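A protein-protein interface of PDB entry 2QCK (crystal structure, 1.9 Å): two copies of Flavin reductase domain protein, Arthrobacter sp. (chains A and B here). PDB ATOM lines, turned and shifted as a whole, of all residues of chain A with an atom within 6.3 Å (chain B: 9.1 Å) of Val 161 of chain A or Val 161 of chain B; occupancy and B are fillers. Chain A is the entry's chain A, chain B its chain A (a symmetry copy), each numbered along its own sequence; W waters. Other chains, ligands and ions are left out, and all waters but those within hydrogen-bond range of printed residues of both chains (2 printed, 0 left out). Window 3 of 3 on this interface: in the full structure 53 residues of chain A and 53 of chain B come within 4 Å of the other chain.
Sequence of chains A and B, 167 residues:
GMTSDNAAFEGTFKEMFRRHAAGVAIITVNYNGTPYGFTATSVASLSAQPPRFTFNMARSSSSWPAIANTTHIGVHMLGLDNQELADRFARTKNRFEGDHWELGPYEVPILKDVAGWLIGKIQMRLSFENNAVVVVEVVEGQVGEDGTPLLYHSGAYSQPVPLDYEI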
ATOM      1  N   LEU A 151       9.052   1.162 -18.818  1.00  0.00           N
ATOM      2  CA  LEU A 151      10.135   0.259 -18.480  1.00  0.00           C
ATOM      3  C   LEU A 151      11.418   1.032 -18.360  1.00  0.00           C
ATOM      4  O   LEU A 151      11.534   2.161 -18.854  1.00  0.00           O
ATOM      5  CB  LEU A 151      10.297  -0.779 -19.566  1.00  0.00           C
ATOM      6  CG  LEU A 151       9.006  -1.296 -20.201  1.00  0.00           C
ATOM      7  CD1 LEU A 151       9.373  -2.035 -21.484  1.00  0.00           C
ATOM      8  CD2 LEU A 151       8.307  -2.165 -19.240  1.00  0.00           C
ATOM      9  N   TYR A 157      14.743   4.823 -20.349  1.00  0.00           N
ATOM     10  CA  TYR A 157      13.318   4.543 -20.321  1.00  0.00           C
ATOM     11  C   TYR A 157      12.892   3.977 -21.658  1.00  0.00           C
ATOM     12  O   TYR A 157      13.214   4.520 -22.693  1.00  0.00           O
ATOM     13  CB  TYR A 157      12.524   5.801 -19.977  1.00  0.00           C
ATOM     14  CG  TYR A 157      12.710   6.243 -18.539  1.00  0.00           C
ATOM     15  CD1 TYR A 157      12.145   5.530 -17.472  1.00  0.00           C
ATOM     16  CD2 TYR A 157      13.446   7.364 -18.237  1.00  0.00           C
ATOM     17  CE1 TYR A 157      12.351   5.952 -16.131  1.00  0.00           C
ATOM     18  CE2 TYR A 157      13.633   7.772 -16.925  1.00  0.00           C
ATOM     19  CZ  TYR A 157      13.098   7.066 -15.892  1.00  0.00           C
ATOM     20  OH  TYR A 157      13.322   7.495 -14.602  1.00  0.00           O
ATOM     21  N   SER A 158      12.127   2.888 -21.616  1.00  0.00           N
ATOM     22  CA  SER A 158      11.714   2.136 -22.773  1.00  0.00           C
ATOM     23  C   SER A 158      10.224   1.854 -22.685  1.00  0.00           C
ATOM     24  O   SER A 158       9.584   2.078 -21.648  1.00  0.00           O
ATOM     25  CB  SER A 158      12.443   0.792 -22.821  1.00  0.00           C
ATOM     26  OG  SER A 158      13.812   0.969 -23.165  1.00  0.00           O
ATOM     27  N   GLN A 159       9.684   1.365 -23.788  1.00  0.00           N
ATOM     28  CA  GLN A 159       8.317   0.924 -23.827  1.00  0.00           C
ATOM     29  C   GLN A 159       8.307  -0.524 -24.304  1.00  0.00           C
ATOM     30  O   GLN A 159       9.181  -0.915 -25.065  1.00  0.00           O
ATOM     31  CB  GLN A 159       7.536   1.798 -24.763  1.00  0.00           C
ATOM     32  CG  GLN A 159       7.830   1.550 -26.224  1.00  0.00           C
ATOM     33  CD  GLN A 159       6.959   2.390 -27.096  1.00  0.00           C
ATOM     34  OE1 GLN A 159       5.733   2.226 -27.102  1.00  0.00           O
ATOM     35  NE2 GLN A 159       7.577   3.307 -27.841  1.00  0.00           N
ATOM     36  N   PRO A 160       7.352  -1.309 -23.823  1.00  0.00           N
ATOM     37  CA  PRO A 160       7.302  -2.694 -24.238  1.00  0.00           C
ATOM     38  C   PRO A 160       6.551  -2.823 -25.562  1.00  0.00           C
ATOM     39  O   PRO A 160       5.515  -2.191 -25.758  1.00  0.00           O
ATOM     40  CB  PRO A 160       6.571  -3.372 -23.094  1.00  0.00           C
ATOM     41  CG  PRO A 160       5.662  -2.361 -22.559  1.00  0.00           C
ATOM     42  CD  PRO A 160       6.279  -0.991 -22.862  1.00  0.00           C
ATOM     43  N   VAL A 161       7.100  -3.600 -26.488  1.00  0.00           N
ATOM     44  CA  VAL A 161       6.390  -3.874 -27.731  1.00  0.00           C
ATOM     45  C   VAL A 161       6.191  -5.365 -27.768  1.00  0.00           C
ATOM     46  O   VAL A 161       7.148  -6.103 -27.657  1.00  0.00           O
ATOM     47  CB  VAL A 161       7.195  -3.461 -28.951  1.00  0.00           C
ATOM     48  CG1 VAL A 161       6.429  -3.848 -30.174  1.00  0.00           C
ATOM     49  CG2 VAL A 161       7.489  -1.990 -28.909  1.00  0.00           C
ATOM     50  N   PRO A 162       4.948  -5.833 -27.856  1.00  0.00           N
ATOM     51  CA  PRO A 162       4.870  -7.285 -27.798  1.00  0.00           C
ATOM     52  C   PRO A 162       5.587  -7.942 -28.948  1.00  0.00           C
ATOM     53  O   PRO A 162       5.778  -7.331 -29.988  1.00  0.00           O
ATOM     54  CB  PRO A 162       3.366  -7.565 -27.835  1.00  0.00           C
ATOM     55  CG  PRO A 162       2.767  -6.349 -28.374  1.00  0.00           C
ATOM     56  CD  PRO A 162       3.617  -5.215 -27.953  1.00  0.00           C
ATOM     57  N   LEU A 163       6.014  -9.176 -28.711  1.00  0.00           N
ATOM     58  CA  LEU A 163       6.697  -9.955 -29.705  1.00  0.00           C
ATOM     59  C   LEU A 163       5.680 -10.548 -30.689  1.00  0.00           C
ATOM     60  O   LEU A 163       4.518 -10.816 -30.345  1.00  0.00           O
ATOM     61  CB  LEU A 163       7.523 -11.042 -29.021  1.00  0.00           C
ATOM     62  CG  LEU A 163       8.630 -10.587 -28.091  1.00  0.00           C
ATOM     63  CD1 LEU A 163       9.258 -11.819 -27.409  1.00  0.00           C
ATOM     64  CD2 LEU A 163       9.675  -9.863 -28.855  1.00  0.00           C
ATOM     65  N   ALA B  21       5.014  -3.814 -15.851  1.00  0.00           N
ATOM     66  CA  ALA B  21       5.836  -4.711 -16.675  1.00  0.00           C
ATOM     67  C   ALA B  21       7.025  -5.250 -15.868  1.00  0.00           C
ATOM     68  O   ALA B  21       7.372  -4.747 -14.786  1.00  0.00           O
ATOM     69  CB  ALA B  21       6.337  -3.965 -17.896  1.00  0.00           C
ATOM     70  N   LEU B  80      15.548 -11.969 -25.942  1.00  0.00           N
ATOM     71  CA  LEU B  80      14.462 -12.322 -26.841  1.00  0.00           C
ATOM     72  C   LEU B  80      14.608 -13.696 -27.449  1.00  0.00           C
ATOM     73  O   LEU B  80      13.613 -14.364 -27.676  1.00  0.00           O
ATOM     74  CB  LEU B  80      14.363 -11.307 -27.966  1.00  0.00           C
ATOM     75  CG  LEU B  80      14.150  -9.872 -27.560  1.00  0.00           C
ATOM     76  CD1 LEU B  80      13.645  -9.097 -28.766  1.00  0.00           C
ATOM     77  CD2 LEU B  80      13.176  -9.749 -26.415  1.00  0.00           C
ATOM     78  N   THR B 148      18.803  -8.256 -26.577  1.00  0.00           N
ATOM     79  CA  THR B 148      17.728  -7.423 -26.056  1.00  0.00           C
ATOM     80  C   THR B 148      17.025  -8.196 -24.933  1.00  0.00           C
ATOM     81  O   THR B 148      16.656  -9.364 -25.107  1.00  0.00           O
ATOM     82  CB  THR B 148      16.770  -7.093 -27.223  1.00  0.00           C
ATOM     83  OG1 THR B 148      17.492  -6.321 -28.192  1.00  0.00           O
ATOM     84  CG2 THR B 148      15.517  -6.346 -26.785  1.00  0.00           C
ATOM     85  N   PRO B 149      16.858  -7.570 -23.771  1.00  0.00           N
ATOM     86  CA  PRO B 149      16.172  -8.253 -22.664  1.00  0.00           C
ATOM     87  C   PRO B 149      14.752  -8.684 -22.972  1.00  0.00           C
ATOM     88  O   PRO B 149      14.054  -8.032 -23.728  1.00  0.00           O
ATOM     89  CB  PRO B 149      16.140  -7.211 -21.552  1.00  0.00           C
ATOM     90  CG  PRO B 149      17.172  -6.212 -21.899  1.00  0.00           C
ATOM     91  CD  PRO B 149      17.338  -6.227 -23.385  1.00  0.00           C
ATOM     92  N   LEU B 150      14.345  -9.795 -22.381  1.00  0.00           N
ATOM     93  CA  LEU B 150      12.960 -10.260 -22.453  1.00  0.00           C
ATOM     94  C   LEU B 150      12.147  -9.651 -21.311  1.00  0.00           C
ATOM     95  O   LEU B 150      12.569  -9.657 -20.127  1.00  0.00           O
ATOM     96  CB  LEU B 150      12.926 -11.793 -22.379  1.00  0.00           C
ATOM     97  CG  LEU B 150      11.628 -12.574 -22.634  1.00  0.00           C
ATOM     98  CD1 LEU B 150      11.143 -12.313 -24.047  1.00  0.00           C
ATOM     99  CD2 LEU B 150      11.878 -14.061 -22.383  1.00  0.00           C
ATOM    100  N   LEU B 151      10.969  -9.150 -21.685  1.00  0.00           N
ATOM    101  CA  LEU B 151      10.020  -8.575 -20.751  1.00  0.00           C
ATOM    102  C   LEU B 151       8.748  -9.375 -20.767  1.00  0.00           C
ATOM    103  O   LEU B 151       8.481 -10.134 -21.709  1.00  0.00           O
ATOM    104  CB  LEU B 151       9.701  -7.154 -21.150  1.00  0.00           C
ATOM    105  CG  LEU B 151      10.868  -6.331 -21.698  1.00  0.00           C
ATOM    106  CD1 LEU B 151      10.294  -5.088 -22.370  1.00  0.00           C
ATOM    107  CD2 LEU B 151      11.785  -5.995 -20.596  1.00  0.00           C
ATOM    108  N   TYR B 152       7.973  -9.235 -19.698  1.00  0.00           N
ATOM    109  CA  TYR B 152       6.649  -9.847 -19.643  1.00  0.00           C
ATOM    110  C   TYR B 152       5.687  -8.832 -19.081  1.00  0.00           C
ATOM    111  O   TYR B 152       5.973  -8.170 -18.092  1.00  0.00           O
ATOM    112  CB  TYR B 152       6.683 -11.005 -18.723  1.00  0.00           C
ATOM    113  CG  TYR B 152       5.472 -11.870 -18.769  1.00  0.00           C
ATOM    114  CD1 TYR B 152       5.269 -12.728 -19.815  1.00  0.00           C
ATOM    115  CD2 TYR B 152       4.508 -11.839 -17.749  1.00  0.00           C
ATOM    116  CE1 TYR B 152       4.191 -13.538 -19.857  1.00  0.00           C
ATOM    117  CE2 TYR B 152       3.389 -12.671 -17.802  1.00  0.00           C
ATOM    118  CZ  TYR B 152       3.253 -13.504 -18.862  1.00  0.00           C
ATOM    119  OH  TYR B 152       2.173 -14.357 -18.954  1.00  0.00           O
ATOM    120  N   HIS B 153       4.554  -8.681 -19.733  1.00  0.00           N
ATOM    121  CA  HIS B 153       3.631  -7.638 -19.384  1.00  0.00           C
ATOM    122  C   HIS B 153       2.249  -8.107 -19.808  1.00  0.00           C
ATOM    123  O   HIS B 153       2.078  -8.635 -20.924  1.00  0.00           O
ATOM    124  CB  HIS B 153       4.002  -6.357 -20.122  1.00  0.00           C
ATOM    125  CG  HIS B 153       2.868  -5.409 -20.273  1.00  0.00           C
ATOM    126  ND1 HIS B 153       2.039  -5.069 -19.219  1.00  0.00           N
ATOM    127  CD2 HIS B 153       2.393  -4.754 -21.355  1.00  0.00           C
ATOM    128  CE1 HIS B 153       1.107  -4.233 -19.644  1.00  0.00           C
ATOM    129  NE2 HIS B 153       1.301  -4.022 -20.935  1.00  0.00           N
ATOM    130  N   ALA B 156       1.934 -11.226 -21.810  1.00  0.00           N
ATOM    131  CA  ALA B 156       2.615 -11.441 -23.078  1.00  0.00           C
ATOM    132  C   ALA B 156       4.090 -11.142 -22.925  1.00  0.00           C
ATOM    133  O   ALA B 156       4.466 -10.251 -22.167  1.00  0.00           O
ATOM    134  CB  ALA B 156       2.006 -10.549 -24.193  1.00  0.00           C
ATOM    135  N   TYR B 157       4.911 -11.911 -23.636  1.00  0.00           N
ATOM    136  CA  TYR B 157       6.326 -11.607 -23.757  1.00  0.00           C
ATOM    137  C   TYR B 157       6.511 -10.449 -24.713  1.00  0.00           C
ATOM    138  O   TYR B 157       5.965 -10.445 -25.795  1.00  0.00           O
ATOM    139  CB  TYR B 157       7.107 -12.834 -24.221  1.00  0.00           C
ATOM    140  CG  TYR B 157       7.185 -13.921 -23.166  1.00  0.00           C
ATOM    141  CD1 TYR B 157       7.982 -13.779 -22.022  1.00  0.00           C
ATOM    142  CD2 TYR B 157       6.466 -15.084 -23.302  1.00  0.00           C
ATOM    143  CE1 TYR B 157       8.022 -14.801 -21.037  1.00  0.00           C
ATOM    144  CE2 TYR B 157       6.519 -16.081 -22.338  1.00  0.00           C
ATOM    145  CZ  TYR B 157       7.281 -15.930 -21.220  1.00  0.00           C
ATOM    146  OH  TYR B 157       7.292 -16.935 -20.279  1.00  0.00           O
ATOM    147  N   SER B 158       7.323  -9.477 -24.304  1.00  0.00           N
ATOM    148  CA  SER B 158       7.539  -8.242 -25.014  1.00  0.00           C
ATOM    149  C   SER B 158       9.030  -7.962 -25.095  1.00  0.00           C
ATOM    150  O   SER B 158       9.848  -8.623 -24.441  1.00  0.00           O
ATOM    151  CB  SER B 158       6.884  -7.078 -24.268  1.00  0.00           C
ATOM    152  OG  SER B 158       5.466  -7.138 -24.379  1.00  0.00           O
ATOM    153  N   GLN B 159       9.367  -6.977 -25.910  1.00  0.00           N
ATOM    154  CA  GLN B 159      10.721  -6.503 -26.000  1.00  0.00           C
ATOM    155  C   GLN B 159      10.711  -5.006 -25.715  1.00  0.00           C
ATOM    156  O   GLN B 159       9.725  -4.342 -26.008  1.00  0.00           O
ATOM    157  CB  GLN B 159      11.258  -6.780 -27.372  1.00  0.00           C
ATOM    158  CG  GLN B 159      10.697  -5.877 -28.445  1.00  0.00           C
ATOM    159  CD  GLN B 159      11.338  -6.151 -29.765  1.00  0.00           C
ATOM    160  OE1 GLN B 159      12.545  -5.943 -29.931  1.00  0.00           O
ATOM    161  NE2 GLN B 159      10.540  -6.629 -30.721  1.00  0.00           N
ATOM    162  N   PRO B 160      11.780  -4.500 -25.115  1.00  0.00           N
ATOM    163  CA  PRO B 160      11.817  -3.085 -24.816  1.00  0.00           C
ATOM    164  C   PRO B 160      12.301  -2.299 -26.033  1.00  0.00           C
ATOM    165  O   PRO B 160      13.245  -2.706 -26.706  1.00  0.00           O
ATOM    166  CB  PRO B 160      12.791  -3.002 -23.654  1.00  0.00           C
ATOM    167  CG  PRO B 160      13.735  -4.098 -23.859  1.00  0.00           C
ATOM    168  CD  PRO B 160      13.003  -5.185 -24.655  1.00  0.00           C
ATOM    169  N   VAL B 161      11.621  -1.202 -26.345  1.00  0.00           N
ATOM    170  CA  VAL B 161      12.087  -0.330 -27.416  1.00  0.00           C
ATOM    171  C   VAL B 161      12.350   1.004 -26.772  1.00  0.00           C
ATOM    172  O   VAL B 161      11.472   1.549 -26.136  1.00  0.00           O
ATOM    173  CB  VAL B 161      11.039  -0.148 -28.500  1.00  0.00           C
ATOM    174  CG1 VAL B 161      11.570   0.816 -29.510  1.00  0.00           C
ATOM    175  CG2 VAL B 161      10.685  -1.472 -29.112  1.00  0.00           C
ATOM    176  N   PRO B 162      13.573   1.519 -26.866  1.00  0.00           N
ATOM    177  CA  PRO B 162      13.735   2.767 -26.136  1.00  0.00           C
ATOM    178  C   PRO B 162      12.841   3.858 -26.664  1.00  0.00           C
ATOM    179  O   PRO B 162      12.420   3.811 -27.810  1.00  0.00           O
ATOM    180  CB  PRO B 162      15.215   3.106 -26.328  1.00  0.00           C
ATOM    181  CG  PRO B 162      15.634   2.330 -27.488  1.00  0.00           C
ATOM    182  CD  PRO B 162      14.827   1.091 -27.506  1.00  0.00           C
ATOM    183  N   LEU B 163      12.531   4.804 -25.787  1.00  0.00           N
ATOM    184  CA  LEU B 163      11.707   5.928 -26.130  1.00  0.00           C
ATOM    185  C   LEU B 163      12.541   6.971 -26.886  1.00  0.00           C
ATOM    186  O   LEU B 163      13.760   7.100 -26.690  1.00  0.00           O
ATOM    187  CB  LEU B 163      11.087   6.511 -24.861  1.00  0.00           C
ATOM    188  CG  LEU B 163      10.162   5.610 -24.067  1.00  0.00           C
ATOM    189  CD1 LEU B 163       9.743   6.331 -22.770  1.00  0.00           C
ATOM    190  CD2 LEU B 163       8.953   5.289 -24.863  1.00  0.00           C
ATOM    191  N   ASP B 164      11.908   7.708 -27.783  1.00  0.00           N
ATOM    192  CA  ASP B 164      12.661   8.636 -28.597  1.00  0.00           C
ATOM    193  C   ASP B 164      13.416   9.584 -27.718  1.00  0.00           C
ATOM    194  O   ASP B 164      12.871  10.025 -26.740  1.00  0.00           O
ATOM    195  CB  ASP B 164      11.720   9.468 -29.469  1.00  0.00           C
ATOM    196  CG  ASP B 164      11.034   8.654 -30.577  1.00  0.00           C
ATOM    197  OD1 ASP B 164      11.389   7.468 -30.838  1.00  0.00           O
ATOM    198  OD2 ASP B 164      10.116   9.239 -31.187  1.00  0.00           O
HETATM  199  O   HOH W   1       8.167  -6.984 -31.224  1.00  0.00           O
HETATM  200  O   HOH W   2       9.820   3.979 -28.566  1.00  0.00           O
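O of Tyr 157 of chain A sits at hydrogen-bond distance from N of Leu 163 of chain B (3.2 Å). N of Val 161 of chain B sits at hydrogen-bond distance from O of Gln 159 of chain A (2.8 Å). N of Val 161 of chain A is in hydrogen-bond range of O of Gln 159 of chain B, 2.8 Å away. The backbone NH (N) of Leu 163 of chain A sits at hydrogen-bond distance from the backbone carbonyl oxygen (O) of Tyr 157 of chain B, 3.2 Å away.
O of Leu 151 of chain A lies within hydrogen-bond range of N of Ser 158 of chain A (2.9 Å). The backbone NH of Ser 158 of chain B sits at hydrogen-bond distance from the backbone carbonyl oxygen of Leu 151 of chain B, 2.9 Å away.
Among the printed residues, pairs that only touch across the chains: Leu 151 of chain A with Ala 21 of chain B (3.0 Å), Val 161 of chain A with Val 161 of chain B (3.2 Å), Leu 151 of chain A with Leu 151 of chain B (3.3 Å), Ser 158 of chain A with Val 161 of chain B (3.4 Å), Val 161 of chain A with Ser 158 of chain B (3.4 Å), Gln 159 of chain A with Pro 160 of chain B (3.4 Å), Pro 160 of chain A with Gln 159 of chain B (3.4 Å), Ser 158 of chain A with Pro 162 of chain B (3.5 Å), Pro 162 of chain A with Ser 158 of chain B (3.5 Å), Gln 159 of chain A with Gln 159 of chain B (3.6 Å), Gln 159 of chain A with Leu 163 of chain B (3.8 Å), Leu 163 of chain A with Gln 159 of chain B (3.8 Å), Leu 163 of chain A with Leu 150 of chain B (3.9 Å), Pro 162 of chain A with Tyr 157 of chain B (3.9 Å), Tyr 157 of chain A with Pro 162 of chain B (3.9 Å), Ser 158 of chain A with Pro 160 of chain B (3.9 Å) and Pro 160 of chain A with Ser 158 of chain B (3.9 Å).
Of the printed residues of chain B, Leu 151 of chain A touches Ala 21 and Leu 151. Of the printed residues of chain B, Tyr 157 of chain A touches Pro 162 (3.9 Å) and Leu 163 (3.2 Å). Gln 159 of chain A touches just these residues of chain B: Gln 159, Pro 160, Val 161 and Leu 163. Pro 160 of chain A touches just these residues of chain B: Ser 158 (3.9 Å) and Gln 159 (3.4 Å). Val 161 of chain A touches just these residues of chain B: Ser 158 (3.4 Å), Gln 159 (2.8 Å) and Val 161 (3.2 Å). Pro 162 of chain A touches just these residues of chain B: Tyr 157 and Ser 158. Thr 148 of chain B touches none of the printed residues of chain A. Of the printed residues of chain A, Ser 158 of chain B touches Pro 160 (3.9 Å), Val 161 (3.4 Å) and Pro 162 (3.5 Å). Of the printed residues of chain A, Gln 159 of chain B touches Gln 159, Pro 160, Val 161 and Leu 163. Val 161 of chain B touches just these residues of chain A: Ser 158 (3.4 Å), Gln 159 (2.8 Å) and Val 161 (3.2 Å). The nearest residue of chain A that does not touch Val 161 of chain B is Tyr 157 of chain A (4.9 Å).
Printed residues of chain A that touch a printed residue of chain B: Leu 151, Tyr 157, Ser 158, Gln 159, Pro 160, Val 161, Pro 162 and Leu 163. Of the 17 printed residues of chain B, 10 touch a printed residue of chain A. Printed residues of chain B that touch a printed residue of chain A: Ala 21, Leu 150, Leu 151, Tyr 157, Ser 158, Gln 159, Pro 160, Val 161, Pro 162 and Leu 163. Hydrophobic or aromatic side chains of chain B that line the printed part of chain A: Ala 21, Leu 150, Leu 151, Tyr 157, Pro 160, Val 161 and Leu 163.
Ser 158 of chain A touches Pro 162 of chain B, and with the chains exchanged Pro 162 of chain A touches Ser 158 of chain B. Gln 159 of chain B touches its own counterpart, Gln 159 of chain A. Gln 159 of chain A touches Pro 160 of chain B, and with the chains exchanged Pro 160 of chain A touches Gln 159 of chain B. Gln 159 of chain A touches Val 161 of chain B, and with the chains exchanged Val 161 of chain A touches Gln 159 of chain B. 8 positions are printed for both chains. Of the 21 pairs that touch across the chains among the printed residues, 19 have their exchanged pair printed and touching as well.
Water W2 lies within hydrogen-bond range of NE2 of Gln 159 of chain A and O of Pro 162 of chain B. Water W1 bridges NE2 of Gln 159 of chain B (2.5 Å) and O of Pro 162 of chain A (2.7 Å).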
